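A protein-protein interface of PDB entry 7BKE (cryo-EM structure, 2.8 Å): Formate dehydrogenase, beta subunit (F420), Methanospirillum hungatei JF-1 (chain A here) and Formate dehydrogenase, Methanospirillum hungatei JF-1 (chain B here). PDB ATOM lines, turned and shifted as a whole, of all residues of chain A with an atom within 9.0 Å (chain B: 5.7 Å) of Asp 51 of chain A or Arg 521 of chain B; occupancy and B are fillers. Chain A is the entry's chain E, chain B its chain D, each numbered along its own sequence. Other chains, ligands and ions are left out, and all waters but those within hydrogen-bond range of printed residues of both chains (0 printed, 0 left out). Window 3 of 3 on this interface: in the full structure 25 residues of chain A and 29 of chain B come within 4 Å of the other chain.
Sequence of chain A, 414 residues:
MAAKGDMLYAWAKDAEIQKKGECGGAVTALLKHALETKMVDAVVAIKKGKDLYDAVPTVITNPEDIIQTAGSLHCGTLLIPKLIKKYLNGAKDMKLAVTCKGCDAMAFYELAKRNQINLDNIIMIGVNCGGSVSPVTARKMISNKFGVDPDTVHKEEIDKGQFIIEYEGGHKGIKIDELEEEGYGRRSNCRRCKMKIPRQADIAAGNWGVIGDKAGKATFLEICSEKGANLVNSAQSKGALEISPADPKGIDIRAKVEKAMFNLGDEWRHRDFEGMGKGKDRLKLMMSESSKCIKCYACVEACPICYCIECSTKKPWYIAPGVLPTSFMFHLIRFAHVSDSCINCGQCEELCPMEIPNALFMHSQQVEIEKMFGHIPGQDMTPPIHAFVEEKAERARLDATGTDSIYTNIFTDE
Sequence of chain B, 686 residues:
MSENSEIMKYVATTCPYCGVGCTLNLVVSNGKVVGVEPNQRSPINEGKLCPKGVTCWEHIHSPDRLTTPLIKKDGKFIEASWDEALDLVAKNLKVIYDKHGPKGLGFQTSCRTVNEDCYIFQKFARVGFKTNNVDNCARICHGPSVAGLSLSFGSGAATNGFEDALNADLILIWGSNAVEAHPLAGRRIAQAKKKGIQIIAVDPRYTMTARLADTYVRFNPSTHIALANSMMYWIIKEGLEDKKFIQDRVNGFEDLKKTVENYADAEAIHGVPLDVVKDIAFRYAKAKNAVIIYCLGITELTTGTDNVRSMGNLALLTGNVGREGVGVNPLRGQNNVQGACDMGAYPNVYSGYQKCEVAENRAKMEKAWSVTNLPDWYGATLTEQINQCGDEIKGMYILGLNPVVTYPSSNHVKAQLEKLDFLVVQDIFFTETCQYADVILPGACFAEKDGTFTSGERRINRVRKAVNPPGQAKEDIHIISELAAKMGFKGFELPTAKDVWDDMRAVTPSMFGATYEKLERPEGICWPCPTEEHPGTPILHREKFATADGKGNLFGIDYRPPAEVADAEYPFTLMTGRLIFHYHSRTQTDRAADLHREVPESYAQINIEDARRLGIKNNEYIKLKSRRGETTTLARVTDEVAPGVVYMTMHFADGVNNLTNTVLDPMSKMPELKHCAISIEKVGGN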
ATOM      1  N   LYS A  47     -11.249  25.842   5.034  1.00  0.00           N
ATOM      2  CA  LYS A  47     -11.963  26.778   4.195  1.00  0.00           C
ATOM      3  C   LYS A  47     -13.386  26.280   4.008  1.00  0.00           C
ATOM      4  O   LYS A  47     -13.676  25.098   4.189  1.00  0.00           O
ATOM      5  CB  LYS A  47     -11.283  26.947   2.838  1.00  0.00           C
ATOM      6  CG  LYS A  47     -11.517  25.783   1.929  1.00  0.00           C
ATOM      7  CD  LYS A  47     -10.979  26.036   0.550  1.00  0.00           C
ATOM      8  CE  LYS A  47     -11.289  24.868  -0.367  1.00  0.00           C
ATOM      9  NZ  LYS A  47     -10.615  25.018  -1.681  1.00  0.00           N
ATOM     10  N   LYS A  48     -14.281  27.194   3.665  1.00  0.00           N
ATOM     11  CA  LYS A  48     -15.635  26.802   3.314  1.00  0.00           C
ATOM     12  C   LYS A  48     -15.636  26.239   1.903  1.00  0.00           C
ATOM     13  O   LYS A  48     -15.081  26.849   0.988  1.00  0.00           O
ATOM     14  CB  LYS A  48     -16.579  27.993   3.408  1.00  0.00           C
ATOM     15  CG  LYS A  48     -16.243  28.950   4.520  1.00  0.00           C
ATOM     16  CD  LYS A  48     -17.257  30.066   4.618  1.00  0.00           C
ATOM     17  CE  LYS A  48     -17.074  31.074   3.511  1.00  0.00           C
ATOM     18  NZ  LYS A  48     -18.063  32.176   3.625  1.00  0.00           N
ATOM     19  N   GLY A  49     -16.244  25.077   1.726  1.00  0.00           N
ATOM     20  CA  GLY A  49     -16.336  24.510   0.397  1.00  0.00           C
ATOM     21  C   GLY A  49     -17.612  24.943  -0.286  1.00  0.00           C
ATOM     22  O   GLY A  49     -17.719  24.971  -1.513  1.00  0.00           O
ATOM     23  N   LYS A  50     -18.582  25.307   0.536  1.00  0.00           N
ATOM     24  CA  LYS A  50     -19.947  25.615   0.142  1.00  0.00           C
ATOM     25  C   LYS A  50     -20.461  26.641   1.137  1.00  0.00           C
ATOM     26  O   LYS A  50     -19.684  27.467   1.625  1.00  0.00           O
ATOM     27  CB  LYS A  50     -20.817  24.364   0.106  1.00  0.00           C
ATOM     28  CG  LYS A  50     -20.717  23.604  -1.198  1.00  0.00           C
ATOM     29  CD  LYS A  50     -21.530  22.327  -1.177  1.00  0.00           C
ATOM     30  CE  LYS A  50     -21.559  21.689  -2.554  1.00  0.00           C
ATOM     31  NZ  LYS A  50     -22.405  20.470  -2.604  1.00  0.00           N
ATOM     32  N   ASP A  51     -21.764  26.651   1.387  1.00  0.00           N
ATOM     33  CA  ASP A  51     -22.317  27.452   2.471  1.00  0.00           C
ATOM     34  C   ASP A  51     -21.469  27.319   3.731  1.00  0.00           C
ATOM     35  O   ASP A  51     -20.792  26.305   3.921  1.00  0.00           O
ATOM     36  CB  ASP A  51     -23.760  27.027   2.744  1.00  0.00           C
ATOM     37  CG  ASP A  51     -23.898  25.534   2.954  1.00  0.00           C
ATOM     38  OD1 ASP A  51     -25.033  25.050   3.138  1.00  0.00           O
ATOM     39  OD2 ASP A  51     -22.871  24.836   2.929  1.00  0.00           O
ATOM     40  N   LEU A  52     -21.492  28.331   4.597  1.00  0.00           N
ATOM     41  CA  LEU A  52     -20.605  28.365   5.756  1.00  0.00           C
ATOM     42  C   LEU A  52     -20.782  27.185   6.692  1.00  0.00           C
ATOM     43  O   LEU A  52     -20.055  27.085   7.684  1.00  0.00           O
ATOM     44  CB  LEU A  52     -20.791  29.663   6.555  1.00  0.00           C
ATOM     45  CG  LEU A  52     -22.048  29.879   7.389  1.00  0.00           C
ATOM     46  CD1 LEU A  52     -21.831  31.001   8.350  1.00  0.00           C
ATOM     47  CD2 LEU A  52     -23.154  30.272   6.457  1.00  0.00           C
ATOM     48  N   TYR A  53     -21.699  26.282   6.408  1.00  0.00           N
ATOM     49  CA  TYR A  53     -21.853  25.100   7.235  1.00  0.00           C
ATOM     50  C   TYR A  53     -20.943  23.971   6.800  1.00  0.00           C
ATOM     51  O   TYR A  53     -20.865  22.959   7.492  1.00  0.00           O
ATOM     52  CB  TYR A  53     -23.301  24.627   7.221  1.00  0.00           C
ATOM     53  CG  TYR A  53     -24.354  25.645   7.608  1.00  0.00           C
ATOM     54  CD1 TYR A  53     -25.544  25.229   8.136  1.00  0.00           C
ATOM     55  CD2 TYR A  53     -24.141  27.011   7.505  1.00  0.00           C
ATOM     56  CE1 TYR A  53     -26.513  26.128   8.494  1.00  0.00           C
ATOM     57  CE2 TYR A  53     -25.104  27.908   7.874  1.00  0.00           C
ATOM     58  CZ  TYR A  53     -26.285  27.458   8.370  1.00  0.00           C
ATOM     59  OH  TYR A  53     -27.255  28.347   8.737  1.00  0.00           O
ATOM     60  N   ASP A  54     -20.239  24.136   5.689  1.00  0.00           N
ATOM     61  CA  ASP A  54     -19.369  23.116   5.123  1.00  0.00           C
ATOM     62  C   ASP A  54     -17.934  23.557   5.350  1.00  0.00           C
ATOM     63  O   ASP A  54     -17.494  24.556   4.784  1.00  0.00           O
ATOM     64  CB  ASP A  54     -19.657  22.931   3.638  1.00  0.00           C
ATOM     65  CG  ASP A  54     -19.359  21.531   3.148  1.00  0.00           C
ATOM     66  OD1 ASP A  54     -19.997  21.093   2.171  1.00  0.00           O
ATOM     67  OD2 ASP A  54     -18.486  20.865   3.737  1.00  0.00           O
ATOM     68  N   ALA A  55     -17.208  22.818   6.178  1.00  0.00           N
ATOM     69  CA  ALA A  55     -15.808  23.095   6.457  1.00  0.00           C
ATOM     70  C   ALA A  55     -14.968  22.017   5.801  1.00  0.00           C
ATOM     71  O   ALA A  55     -15.157  20.830   6.076  1.00  0.00           O
ATOM     72  CB  ALA A  55     -15.546  23.141   7.957  1.00  0.00           C
ATOM     73  N   VAL A  56     -14.042  22.427   4.947  1.00  0.00           N
ATOM     74  CA  VAL A  56     -13.239  21.518   4.144  1.00  0.00           C
ATOM     75  C   VAL A  56     -11.773  21.780   4.462  1.00  0.00           C
ATOM     76  O   VAL A  56     -11.305  22.909   4.310  1.00  0.00           O
ATOM     77  CB  VAL A  56     -13.507  21.694   2.641  1.00  0.00           C
ATOM     78  CG1 VAL A  56     -12.768  20.662   1.851  1.00  0.00           C
ATOM     79  CG2 VAL A  56     -14.978  21.591   2.362  1.00  0.00           C
ATOM     80  N   LEU A  73     -15.017  28.825  11.130  1.00  0.00           N
ATOM     81  CA  LEU A  73     -16.254  28.066  10.861  1.00  0.00           C
ATOM     82  C   LEU A  73     -16.587  27.304  12.130  1.00  0.00           C
ATOM     83  O   LEU A  73     -15.813  26.438  12.491  1.00  0.00           O
ATOM     84  CB  LEU A  73     -15.999  27.104   9.703  1.00  0.00           C
ATOM     85  CG  LEU A  73     -15.885  27.715   8.314  1.00  0.00           C
ATOM     86  CD1 LEU A  73     -14.450  27.656   7.832  1.00  0.00           C
ATOM     87  CD2 LEU A  73     -16.783  26.957   7.359  1.00  0.00           C
ATOM     88  N   CYS A  75     -19.051  25.425  12.523  1.00  0.00           N
ATOM     89  CA  CYS A  75     -19.589  24.124  12.173  1.00  0.00           C
ATOM     90  C   CYS A  75     -18.510  23.167  11.708  1.00  0.00           C
ATOM     91  O   CYS A  75     -18.823  22.071  11.249  1.00  0.00           O
ATOM     92  CB  CYS A  75     -20.665  24.271  11.105  1.00  0.00           C
ATOM     93  SG  CYS A  75     -22.259  24.778  11.766  1.00  0.00           S
ATOM     94  N   PRO A 135     -22.940  20.537  11.561  1.00  0.00           N
ATOM     95  CA  PRO A 135     -23.599  21.386  10.560  1.00  0.00           C
ATOM     96  C   PRO A 135     -25.083  21.123  10.418  1.00  0.00           C
ATOM     97  O   PRO A 135     -25.877  22.066  10.352  1.00  0.00           O
ATOM     98  CB  PRO A 135     -22.838  21.047   9.277  1.00  0.00           C
ATOM     99  CG  PRO A 135     -21.534  20.541   9.729  1.00  0.00           C
ATOM    100  CD  PRO A 135     -21.795  19.808  10.994  1.00  0.00           C
ATOM    101  N   VAL A 136     -25.487  19.860  10.380  1.00  0.00           N
ATOM    102  CA  VAL A 136     -26.893  19.538  10.183  1.00  0.00           C
ATOM    103  C   VAL A 136     -27.706  19.904  11.416  1.00  0.00           C
ATOM    104  O   VAL A 136     -28.846  20.375  11.312  1.00  0.00           O
ATOM    105  CB  VAL A 136     -27.031  18.056   9.810  1.00  0.00           C
ATOM    106  CG1 VAL A 136     -28.442  17.583  10.008  1.00  0.00           C
ATOM    107  CG2 VAL A 136     -26.612  17.856   8.378  1.00  0.00           C
ATOM    108  N   ARG A 139     -28.295  23.512  11.265  1.00  0.00           N
ATOM    109  CA  ARG A 139     -29.398  23.781  10.346  1.00  0.00           C
ATOM    110  C   ARG A 139     -30.747  23.578  11.015  1.00  0.00           C
ATOM    111  O   ARG A 139     -31.638  24.423  10.887  1.00  0.00           O
ATOM    112  CB  ARG A 139     -29.298  22.888   9.116  1.00  0.00           C
ATOM    113  CG  ARG A 139     -28.248  23.310   8.137  1.00  0.00           C
ATOM    114  CD  ARG A 139     -28.382  22.569   6.835  1.00  0.00           C
ATOM    115  NE  ARG A 139     -29.477  23.051   6.001  1.00  0.00           N
ATOM    116  CZ  ARG A 139     -29.409  24.126   5.227  1.00  0.00           C
ATOM    117  NH1 ARG A 139     -28.302  24.850   5.190  1.00  0.00           N
ATOM    118  NH2 ARG A 139     -30.450  24.481   4.495  1.00  0.00           N
ATOM    119  N   PRO A 150     -32.336  28.422   6.943  1.00  0.00           N
ATOM    120  CA  PRO A 150     -30.889  28.359   7.194  1.00  0.00           C
ATOM    121  C   PRO A 150     -30.045  28.873   6.052  1.00  0.00           C
ATOM    122  O   PRO A 150     -28.914  29.305   6.287  1.00  0.00           O
ATOM    123  CB  PRO A 150     -30.640  26.868   7.441  1.00  0.00           C
ATOM    124  CG  PRO A 150     -31.955  26.307   7.761  1.00  0.00           C
ATOM    125  CD  PRO A 150     -32.949  27.089   6.985  1.00  0.00           C
ATOM    126  N   ASP A 151     -30.546  28.832   4.821  1.00  0.00           N
ATOM    127  CA  ASP A 151     -29.774  29.309   3.683  1.00  0.00           C
ATOM    128  C   ASP A 151     -29.628  30.822   3.669  1.00  0.00           C
ATOM    129  O   ASP A 151     -28.798  31.346   2.921  1.00  0.00           O
ATOM    130  CB  ASP A 151     -30.423  28.832   2.392  1.00  0.00           C
ATOM    131  CG  ASP A 151     -30.127  27.380   2.115  1.00  0.00           C
ATOM    132  OD1 ASP A 151     -28.965  26.970   2.324  1.00  0.00           O
ATOM    133  OD2 ASP A 151     -31.048  26.649   1.695  1.00  0.00           O
ATOM    134  N   THR A 152     -30.406  31.522   4.483  1.00  0.00           N
ATOM    135  CA  THR A 152     -30.352  32.972   4.573  1.00  0.00           C
ATOM    136  C   THR A 152     -29.150  33.460   5.374  1.00  0.00           C
ATOM    137  O   THR A 152     -28.620  34.539   5.091  1.00  0.00           O
ATOM    138  CB  THR A 152     -31.662  33.456   5.184  1.00  0.00           C
ATOM    139  OG1 THR A 152     -32.713  33.299   4.224  1.00  0.00           O
ATOM    140  CG2 THR A 152     -31.576  34.877   5.604  1.00  0.00           C
ATOM    141  N   VAL A 153     -28.684  32.666   6.338  1.00  0.00           N
ATOM    142  CA  VAL A 153     -27.628  33.105   7.243  1.00  0.00           C
ATOM    143  C   VAL A 153     -26.352  33.441   6.484  1.00  0.00           C
ATOM    144  O   VAL A 153     -25.932  32.712   5.579  1.00  0.00           O
ATOM    145  CB  VAL A 153     -27.371  32.016   8.292  1.00  0.00           C
ATOM    146  CG1 VAL A 153     -26.380  32.493   9.316  1.00  0.00           C
ATOM    147  CG2 VAL A 153     -28.666  31.616   8.952  1.00  0.00           C
ATOM    148  N   HIS A 154     -25.724  34.556   6.855  1.00  0.00           N
ATOM    149  CA  HIS A 154     -24.414  34.929   6.332  1.00  0.00           C
ATOM    150  C   HIS A 154     -23.292  34.431   7.234  1.00  0.00           C
ATOM    151  O   HIS A 154     -22.427  33.672   6.794  1.00  0.00           O
ATOM    152  CB  HIS A 154     -24.293  36.447   6.168  1.00  0.00           C
ATOM    153  CG  HIS A 154     -25.435  37.077   5.440  1.00  0.00           C
ATOM    154  ND1 HIS A 154     -26.227  36.382   4.554  1.00  0.00           N
ATOM    155  CD2 HIS A 154     -25.916  38.340   5.464  1.00  0.00           C
ATOM    156  CE1 HIS A 154     -27.150  37.191   4.065  1.00  0.00           C
ATOM    157  NE2 HIS A 154     -26.982  38.387   4.602  1.00  0.00           N
ATOM    158  N   GLU A 156     -22.328  33.279  11.584  1.00  0.00           N
ATOM    159  CA  GLU A 156     -22.894  32.684  12.784  1.00  0.00           C
ATOM    160  C   GLU A 156     -21.773  32.299  13.731  1.00  0.00           C
ATOM    161  O   GLU A 156     -20.771  31.720  13.310  1.00  0.00           O
ATOM    162  CB  GLU A 156     -23.798  31.499  12.417  1.00  0.00           C
ATOM    163  CG  GLU A 156     -23.123  30.362  11.677  1.00  0.00           C
ATOM    164  CD  GLU A 156     -22.457  29.348  12.566  1.00  0.00           C
ATOM    165  OE1 GLU A 156     -22.797  29.285  13.759  1.00  0.00           O
ATOM    166  OE2 GLU A 156     -21.594  28.604  12.061  1.00  0.00           O
ATOM    167  N   ARG B  41     -21.547  17.689   6.146  1.00  0.00           N
ATOM    168  CA  ARG B  41     -22.571  18.622   5.705  1.00  0.00           C
ATOM    169  C   ARG B  41     -23.811  17.900   5.193  1.00  0.00           C
ATOM    170  O   ARG B  41     -24.914  18.446   5.262  1.00  0.00           O
ATOM    171  CB  ARG B  41     -21.988  19.530   4.632  1.00  0.00           C
ATOM    172  CG  ARG B  41     -22.962  20.479   4.008  1.00  0.00           C
ATOM    173  CD  ARG B  41     -23.598  21.366   5.039  1.00  0.00           C
ATOM    174  NE  ARG B  41     -24.443  22.359   4.404  1.00  0.00           N
ATOM    175  CZ  ARG B  41     -25.719  22.166   4.109  1.00  0.00           C
ATOM    176  NH1 ARG B  41     -26.307  21.020   4.407  1.00  0.00           N
ATOM    177  NH2 ARG B  41     -26.407  23.127   3.523  1.00  0.00           N
ATOM    178  N   TYR B 516     -28.755  21.805 -12.493  1.00  0.00           N
ATOM    179  CA  TYR B 516     -27.554  21.570 -11.692  1.00  0.00           C
ATOM    180  C   TYR B 516     -27.229  22.711 -10.745  1.00  0.00           C
ATOM    181  O   TYR B 516     -26.632  22.469  -9.694  1.00  0.00           O
ATOM    182  CB  TYR B 516     -26.310  21.258 -12.521  1.00  0.00           C
ATOM    183  CG  TYR B 516     -26.311  19.931 -13.210  1.00  0.00           C
ATOM    184  CD1 TYR B 516     -27.230  18.966 -12.871  1.00  0.00           C
ATOM    185  CD2 TYR B 516     -25.253  19.555 -14.011  1.00  0.00           C
ATOM    186  CE1 TYR B 516     -27.194  17.728 -13.430  1.00  0.00           C
ATOM    187  CE2 TYR B 516     -25.200  18.311 -14.563  1.00  0.00           C
ATOM    188  CZ  TYR B 516     -26.175  17.400 -14.269  1.00  0.00           C
ATOM    189  OH  TYR B 516     -26.140  16.150 -14.819  1.00  0.00           O
ATOM    190  N   GLU B 517     -27.577  23.948 -11.076  1.00  0.00           N
ATOM    191  CA  GLU B 517     -27.367  25.007 -10.099  1.00  0.00           C
ATOM    192  C   GLU B 517     -28.177  24.757  -8.840  1.00  0.00           C
ATOM    193  O   GLU B 517     -27.811  25.231  -7.762  1.00  0.00           O
ATOM    194  CB  GLU B 517     -27.703  26.363 -10.711  1.00  0.00           C
ATOM    195  CG  GLU B 517     -26.807  26.719 -11.877  1.00  0.00           C
ATOM    196  CD  GLU B 517     -27.258  26.089 -13.178  1.00  0.00           C
ATOM    197  OE1 GLU B 517     -28.269  25.359 -13.163  1.00  0.00           O
ATOM    198  OE2 GLU B 517     -26.600  26.318 -14.217  1.00  0.00           O
ATOM    199  N   LYS B 518     -29.264  24.000  -8.952  1.00  0.00           N
ATOM    200  CA  LYS B 518     -30.053  23.599  -7.798  1.00  0.00           C
ATOM    201  C   LYS B 518     -29.573  22.296  -7.177  1.00  0.00           C
ATOM    202  O   LYS B 518     -29.782  22.083  -5.979  1.00  0.00           O
ATOM    203  CB  LYS B 518     -31.521  23.467  -8.192  1.00  0.00           C
ATOM    204  CG  LYS B 518     -32.472  24.050  -7.184  1.00  0.00           C
ATOM    205  CD  LYS B 518     -33.892  23.640  -7.473  1.00  0.00           C
ATOM    206  CE  LYS B 518     -34.504  24.537  -8.508  1.00  0.00           C
ATOM    207  NZ  LYS B 518     -35.929  24.209  -8.723  1.00  0.00           N
ATOM    208  N   LEU B 519     -28.951  21.415  -7.955  1.00  0.00           N
ATOM    209  CA  LEU B 519     -28.413  20.176  -7.410  1.00  0.00           C
ATOM    210  C   LEU B 519     -27.064  20.367  -6.743  1.00  0.00           C
ATOM    211  O   LEU B 519     -26.615  19.469  -6.022  1.00  0.00           O
ATOM    212  CB  LEU B 519     -28.278  19.112  -8.497  1.00  0.00           C
ATOM    213  CG  LEU B 519     -29.502  18.770  -9.326  1.00  0.00           C
ATOM    214  CD1 LEU B 519     -29.132  17.749 -10.356  1.00  0.00           C
ATOM    215  CD2 LEU B 519     -30.586  18.241  -8.445  1.00  0.00           C
ATOM    216  N   GLU B 520     -26.405  21.499  -6.963  1.00  0.00           N
ATOM    217  CA  GLU B 520     -25.180  21.796  -6.234  1.00  0.00           C
ATOM    218  C   GLU B 520     -25.433  22.028  -4.756  1.00  0.00           C
ATOM    219  O   GLU B 520     -24.473  22.127  -3.988  1.00  0.00           O
ATOM    220  CB  GLU B 520     -24.483  23.021  -6.816  1.00  0.00           C
ATOM    221  CG  GLU B 520     -23.965  22.838  -8.226  1.00  0.00           C
ATOM    222  CD  GLU B 520     -22.879  21.795  -8.335  1.00  0.00           C
ATOM    223  OE1 GLU B 520     -22.193  21.534  -7.325  1.00  0.00           O
ATOM    224  OE2 GLU B 520     -22.699  21.242  -9.440  1.00  0.00           O
ATOM    225  N   ARG B 521     -26.687  22.160  -4.346  1.00  0.00           N
ATOM    226  CA  ARG B 521     -26.986  22.210  -2.929  1.00  0.00           C
ATOM    227  C   ARG B 521     -26.729  20.840  -2.315  1.00  0.00           C
ATOM    228  O   ARG B 521     -27.052  19.819  -2.923  1.00  0.00           O
ATOM    229  CB  ARG B 521     -28.436  22.620  -2.684  1.00  0.00           C
ATOM    230  CG  ARG B 521     -28.914  23.842  -3.443  1.00  0.00           C
ATOM    231  CD  ARG B 521     -27.909  24.965  -3.436  1.00  0.00           C
ATOM    232  NE  ARG B 521     -27.425  25.262  -2.094  1.00  0.00           N
ATOM    233  CZ  ARG B 521     -26.164  25.574  -1.818  1.00  0.00           C
ATOM    234  NH1 ARG B 521     -25.268  25.630  -2.796  1.00  0.00           N
ATOM    235  NH2 ARG B 521     -25.800  25.830  -0.571  1.00  0.00           N
ATOM    236  N   PRO B 522     -26.158  20.780  -1.113  1.00  0.00           N
ATOM    237  CA  PRO B 522     -25.952  19.479  -0.466  1.00  0.00           C
ATOM    238  C   PRO B 522     -27.238  18.729  -0.214  1.00  0.00           C
ATOM    239  O   PRO B 522     -27.193  17.511  -0.004  1.00  0.00           O
ATOM    240  CB  PRO B 522     -25.258  19.844   0.845  1.00  0.00           C
ATOM    241  CG  PRO B 522     -24.636  21.163   0.582  1.00  0.00           C
ATOM    242  CD  PRO B 522     -25.554  21.876  -0.346  1.00  0.00           C
ATOM    243  N   GLU B 523     -28.380  19.409  -0.228  1.00  0.00           N
ATOM    244  CA  GLU B 523     -29.652  18.757   0.036  1.00  0.00           C
ATOM    245  C   GLU B 523     -30.140  17.938  -1.149  1.00  0.00           C
ATOM    246  O   GLU B 523     -30.818  16.926  -0.952  1.00  0.00           O
ATOM    247  CB  GLU B 523     -30.702  19.802   0.411  1.00  0.00           C
ATOM    248  CG  GLU B 523     -30.616  20.292   1.843  1.00  0.00           C
ATOM    249  CD  GLU B 523     -29.357  21.094   2.123  1.00  0.00           C
ATOM    250  OE1 GLU B 523     -28.980  21.933   1.278  1.00  0.00           O
ATOM    251  OE2 GLU B 523     -28.743  20.883   3.190  1.00  0.00           O
ATOM    252  N   GLY B 524     -29.794  18.292  -2.387  1.00  0.00           N
ATOM    253  CA  GLY B 524     -30.260  17.560  -3.579  1.00  0.00           C
ATOM    254  C   GLY B 524     -31.667  17.970  -3.938  1.00  0.00           C
ATOM    255  O   GLY B 524     -32.096  18.981  -3.420  1.00  0.00           O
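OD1 of Asp 51 of chain A lies within salt-bridge range of NH2 of Arg 521 of chain B, at 3.9 Å.
The guanidinium group (NE) of Arg 41 of chain B is in salt-bridge range of the side-chain carboxylate (OD1) of Asp 51 of chain A.
NH1 of Arg 139 of chain A sits close to NH2 of Arg 41 of chain B (3.1 Å).
The side-chain amino group (NZ) of Lys 50 of chain A sits at hydrogen-bond distance from the backbone carbonyl oxygen (O) of Glu 520 of chain B (3.0 Å).
NE of Arg 139 of chain A lies within salt-bridge range of OE2 of Glu 523 of chain B (3.6 Å).
The backbone carbonyl oxygen of Pro 150 of chain A is in hydrogen-bond range of the side-chain hydroxyl of Tyr 53 of chain A (3.1 Å).
N of Gly 49 of chain A lies within hydrogen-bond range of O of Asp 54 of chain A, at 3.3 Å.
The guanidinium group of Arg 139 of chain A is in salt-bridge range of the side-chain carboxylate of Asp 51 of chain A.
The guanidinium group (NH2) of Arg 139 of chain A is in salt-bridge range of the side-chain carboxylate (OD2) of Asp 151 of chain A, at 3.6 Å.
The side-chain carboxylate (OE2) of Glu 523 of chain B is in salt-bridge range of the guanidinium group (NH1) of Arg 41 of chain B, at 2.7 Å.
Lys 50 of chain A touches Pro 522 of chain B.
Tyr 53 of chain A touches Arg 41 of chain B (CB to NE, 3.8 Å).
Arg 41 of chain B touches Asp 54 of chain A.
Val 136 of chain A touches Arg 41 of chain B (CG2 to O, 3.6 Å).
Of the printed residues of chain A, Arg 521 of chain B touches Asp 51 (3.9 Å).
Of chain A, only Lys 50 (3.8 Å) comes within 4 Å of Pro 522 of chain B.
Of the printed residues of chain B, Lys 50 of chain A touches Glu 520 (3.0 Å) and Pro 522 (3.8 Å).
Printed residues of chain B within 4 Å of Tyr 53 of chain A: Arg 41 (3.8 Å).
Of the printed residues of chain B, Val 136 of chain A touches Arg 41.
Tyr 516 of chain B touches none of the printed residues of chain A.
Thr 152 of chain A touches none of the printed residues of chain B.
The nearest residue of chain A that does not touch Arg 521 of chain B is Lys 50 of chain A (4.3 Å).
Of the 10 printed residues of chain B, 5 touch a printed residue of chain A.
Hydrophobic or aromatic side chains of chain B within 4 Å of the printed part of chain A: Pro 522.
Of the 21 printed residues of chain A, 6 touch a printed residue of chain B.
Hydrophobic or aromatic side chains of chain A within 4 Å of the printed part of chain B: Tyr 53 and Val 136.
Among the printed residues, 9 pairs touch across the chains.
Among the printed residues, Asp or Glu carboxylates within 4 Å of a Lys or Arg side-chain nitrogen of the other chain: Asp 51 of chain A with Arg 41 of chain B, Asp 51 of chain A with Arg 521 of chain B and Arg 139 of chain A with Glu 523 of chain B.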
